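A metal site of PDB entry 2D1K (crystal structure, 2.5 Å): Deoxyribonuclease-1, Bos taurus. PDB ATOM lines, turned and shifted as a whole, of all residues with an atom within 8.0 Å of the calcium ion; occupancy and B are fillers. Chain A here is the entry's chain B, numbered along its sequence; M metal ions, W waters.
Four residues have an atom within 4 Å of the calcium ion: Asp 201, Thr 203, Thr 205 and Thr 207. The nearest printed residue that does not touch the calcium ion is Ala 204 (4.4 Å).
The side-chain hydroxyl of Thr 205 is in hydrogen-bond range of the side-chain hydroxyl of Thr 207, at 3.1 Å.
The calcium ion is bound by water W2 (2.2 Å), OD1 of Asp 201 (2.3 Å), O of Thr 203 (2.4 Å), O of Thr 207 (2.5 Å), OG1 of Thr 203 (2.5 Å), O of Thr 205 (2.5 Å), water W1 (2.6 Å) and OD2 of Asp 201 (2.7 Å). The calcium ion has eight donor atoms within binding distance.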
ATOM      1  N   ALA A 200     -30.334 -21.581 -24.028  1.00  0.00           N
ATOM      2  CA  ALA A 200     -29.161 -21.827 -23.171  1.00  0.00           C
ATOM      3  C   ALA A 200     -29.074 -20.912 -21.921  1.00  0.00           C
ATOM      4  O   ALA A 200     -29.518 -19.775 -21.938  1.00  0.00           O
ATOM      5  CB  ALA A 200     -27.879 -21.767 -23.980  1.00  0.00           C
ATOM      6  N   ASP A 201     -28.507 -21.436 -20.831  1.00  0.00           N
ATOM      7  CA  ASP A 201     -28.422 -20.724 -19.559  1.00  0.00           C
ATOM      8  C   ASP A 201     -26.934 -20.413 -19.370  1.00  0.00           C
ATOM      9  O   ASP A 201     -26.151 -21.312 -19.052  1.00  0.00           O
ATOM     10  CB  ASP A 201     -28.999 -21.600 -18.427  1.00  0.00           C
ATOM     11  CG  ASP A 201     -28.588 -21.133 -17.008  1.00  0.00           C
ATOM     12  OD1 ASP A 201     -28.546 -19.898 -16.751  1.00  0.00           O
ATOM     13  OD2 ASP A 201     -28.325 -21.980 -16.126  1.00  0.00           O
ATOM     14  N   THR A 202     -26.546 -19.163 -19.593  1.00  0.00           N
ATOM     15  CA  THR A 202     -25.136 -18.792 -19.526  1.00  0.00           C
ATOM     16  C   THR A 202     -24.829 -18.008 -18.235  1.00  0.00           C
ATOM     17  O   THR A 202     -23.760 -17.413 -18.099  1.00  0.00           O
ATOM     18  CB  THR A 202     -24.666 -18.009 -20.787  1.00  0.00           C
ATOM     19  OG1 THR A 202     -25.319 -16.723 -20.866  1.00  0.00           O
ATOM     20  CG2 THR A 202     -24.933 -18.788 -22.085  1.00  0.00           C
ATOM     21  N   THR A 203     -25.749 -18.042 -17.270  1.00  0.00           N
ATOM     22  CA  THR A 203     -25.605 -17.325 -16.013  1.00  0.00           C
ATOM     23  C   THR A 203     -25.417 -18.275 -14.838  1.00  0.00           C
ATOM     24  O   THR A 203     -26.155 -19.276 -14.686  1.00  0.00           O
ATOM     25  CB  THR A 203     -26.881 -16.554 -15.672  1.00  0.00           C
ATOM     26  OG1 THR A 203     -27.878 -17.488 -15.183  1.00  0.00           O
ATOM     27  CG2 THR A 203     -27.390 -15.811 -16.881  1.00  0.00           C
ATOM     28  N   ALA A 204     -24.481 -17.915 -13.957  1.00  0.00           N
ATOM     29  CA  ALA A 204     -24.238 -18.715 -12.764  1.00  0.00           C
ATOM     30  C   ALA A 204     -25.307 -18.488 -11.709  1.00  0.00           C
ATOM     31  O   ALA A 204     -25.364 -19.213 -10.720  1.00  0.00           O
ATOM     32  CB  ALA A 204     -22.843 -18.423 -12.189  1.00  0.00           C
ATOM     33  N   THR A 205     -26.145 -17.479 -11.891  1.00  0.00           N
ATOM     34  CA  THR A 205     -27.204 -17.207 -10.911  1.00  0.00           C
ATOM     35  C   THR A 205     -28.468 -18.066 -11.173  1.00  0.00           C
ATOM     36  O   THR A 205     -28.496 -18.907 -12.053  1.00  0.00           O
ATOM     37  CB  THR A 205     -27.517 -15.713 -10.885  1.00  0.00           C
ATOM     38  OG1 THR A 205     -27.802 -15.269 -12.215  1.00  0.00           O
ATOM     39  CG2 THR A 205     -26.334 -14.924 -10.316  1.00  0.00           C
ATOM     40  N   SER A 206     -29.513 -17.864 -10.391  1.00  0.00           N
ATOM     41  CA  SER A 206     -30.708 -18.664 -10.589  1.00  0.00           C
ATOM     42  C   SER A 206     -31.598 -18.125 -11.741  1.00  0.00           C
ATOM     43  O   SER A 206     -32.728 -18.570 -11.901  1.00  0.00           O
ATOM     44  CB  SER A 206     -31.492 -18.790  -9.299  1.00  0.00           C
ATOM     45  OG  SER A 206     -31.962 -17.527  -8.859  1.00  0.00           O
ATOM     46  N   THR A 207     -31.084 -17.214 -12.540  1.00  0.00           N
ATOM     47  CA  THR A 207     -31.788 -16.823 -13.732  1.00  0.00           C
ATOM     48  C   THR A 207     -31.423 -17.752 -14.874  1.00  0.00           C
ATOM     49  O   THR A 207     -30.297 -18.264 -14.930  1.00  0.00           O
ATOM     50  CB  THR A 207     -31.474 -15.391 -14.131  1.00  0.00           C
ATOM     51  OG1 THR A 207     -30.062 -15.281 -14.388  1.00  0.00           O
ATOM     52  CG2 THR A 207     -31.881 -14.431 -13.006  1.00  0.00           C
ATOM     53  N   ASN A 208     -32.374 -17.963 -15.775  1.00  0.00           N
ATOM     54  CA  ASN A 208     -32.207 -18.788 -16.958  1.00  0.00           C
ATOM     55  C   ASN A 208     -32.120 -17.877 -18.133  1.00  0.00           C
ATOM     56  O   ASN A 208     -33.153 -17.489 -18.653  1.00  0.00           O
ATOM     57  CB  ASN A 208     -33.412 -19.707 -17.168  1.00  0.00           C
ATOM     58  CG  ASN A 208     -33.249 -20.607 -18.393  1.00  0.00           C
ATOM     59  OD1 ASN A 208     -32.127 -20.946 -18.787  1.00  0.00           O
ATOM     60  ND2 ASN A 208     -34.372 -21.026 -18.983  1.00  0.00           N
ATOM     61  N   CYS A 209     -30.915 -17.554 -18.565  1.00  0.00           N
ATOM     62  CA  CYS A 209     -30.764 -16.545 -19.607  1.00  0.00           C
ATOM     63  C   CYS A 209     -29.640 -16.880 -20.548  1.00  0.00           C
ATOM     64  O   CYS A 209     -28.573 -17.346 -20.107  1.00  0.00           O
ATOM     65  CB  CYS A 209     -30.507 -15.161 -18.991  1.00  0.00           C
ATOM     66  SG  CYS A 209     -31.880 -14.432 -18.028  1.00  0.00           S
ATOM     67  N   ASP A 234     -20.579 -24.980 -17.405  1.00  0.00           N
ATOM     68  CA  ASP A 234     -21.086 -24.856 -16.052  1.00  0.00           C
ATOM     69  C   ASP A 234     -20.027 -25.288 -15.076  1.00  0.00           C
ATOM     70  O   ASP A 234     -19.941 -26.471 -14.734  1.00  0.00           O
ATOM     71  CB  ASP A 234     -22.345 -25.701 -15.902  1.00  0.00           C
ATOM     72  CG  ASP A 234     -22.925 -25.612 -14.519  1.00  0.00           C
ATOM     73  OD1 ASP A 234     -22.344 -24.897 -13.661  1.00  0.00           O
ATOM     74  OD2 ASP A 234     -23.947 -26.270 -14.281  1.00  0.00           O
ATOM     75  N   GLN A 236     -19.706 -24.745 -11.908  1.00  0.00           N
ATOM     76  CA  GLN A 236     -20.233 -25.161 -10.608  1.00  0.00           C
ATOM     77  C   GLN A 236     -20.288 -26.673 -10.553  1.00  0.00           C
ATOM     78  O   GLN A 236     -19.681 -27.278  -9.680  1.00  0.00           O
ATOM     79  CB  GLN A 236     -21.601 -24.573 -10.350  1.00  0.00           C
ATOM     80  CG  GLN A 236     -22.109 -24.801  -8.939  1.00  0.00           C
ATOM     81  CD  GLN A 236     -23.378 -24.037  -8.633  1.00  0.00           C
ATOM     82  OE1 GLN A 236     -23.501 -22.873  -8.986  1.00  0.00           O
ATOM     83  NE2 GLN A 236     -24.336 -24.680  -7.973  1.00  0.00           N
ATOM     84  N   ASN A 243     -22.941 -23.045  -4.574  1.00  0.00           N
ATOM     85  CA  ASN A 243     -23.400 -21.853  -5.294  1.00  0.00           C
ATOM     86  C   ASN A 243     -22.598 -20.597  -4.945  1.00  0.00           C
ATOM     87  O   ASN A 243     -22.125 -19.883  -5.832  1.00  0.00           O
ATOM     88  CB  ASN A 243     -24.879 -21.609  -5.001  1.00  0.00           C
ATOM     89  CG  ASN A 243     -25.700 -21.345  -6.250  1.00  0.00           C
ATOM     90  OD1 ASN A 243     -26.891 -21.673  -6.287  1.00  0.00           O
ATOM     91  ND2 ASN A 243     -25.075 -20.770  -7.281  1.00  0.00           N
ATOM     92  N   ASP A 251     -20.736 -14.372 -12.243  1.00  0.00           N
ATOM     93  CA  ASP A 251     -22.170 -14.666 -12.359  1.00  0.00           C
ATOM     94  C   ASP A 251     -22.539 -15.148 -13.780  1.00  0.00           C
ATOM     95  O   ASP A 251     -23.709 -15.425 -14.114  1.00  0.00           O
ATOM     96  CB  ASP A 251     -23.049 -13.528 -11.819  1.00  0.00           C
ATOM     97  CG  ASP A 251     -22.710 -12.197 -12.422  1.00  0.00           C
ATOM     98  OD1 ASP A 251     -21.882 -12.136 -13.346  1.00  0.00           O
ATOM     99  OD2 ASP A 251     -23.292 -11.179 -11.967  1.00  0.00           O
ATOM    100  N   TYR A 253     -21.228 -18.069 -16.852  1.00  0.00           N
ATOM    101  CA  TYR A 253     -20.449 -19.164 -17.365  1.00  0.00           C
ATOM    102  C   TYR A 253     -19.742 -18.692 -18.645  1.00  0.00           C
ATOM    103  O   TYR A 253     -20.307 -17.882 -19.399  1.00  0.00           O
ATOM    104  CB  TYR A 253     -21.403 -20.269 -17.722  1.00  0.00           C
ATOM    105  CG  TYR A 253     -22.203 -20.808 -16.561  1.00  0.00           C
ATOM    106  CD1 TYR A 253     -21.577 -21.098 -15.335  1.00  0.00           C
ATOM    107  CD2 TYR A 253     -23.556 -21.120 -16.717  1.00  0.00           C
ATOM    108  CE1 TYR A 253     -22.292 -21.630 -14.281  1.00  0.00           C
ATOM    109  CE2 TYR A 253     -24.284 -21.655 -15.667  1.00  0.00           C
ATOM    110  CZ  TYR A 253     -23.645 -21.888 -14.431  1.00  0.00           C
ATOM    111  OH  TYR A 253     -24.329 -22.416 -13.380  1.00  0.00           O
HETATM  112 CA    CA M   1     -28.469 -19.843 -14.421  1.00  0.00          CA
HETATM  113  O   HOH W   1     -30.422 -21.100 -13.253  1.00  0.00           O
HETATM  114  O   HOH W   2     -27.195 -21.455 -13.532  1.00  0.00           O
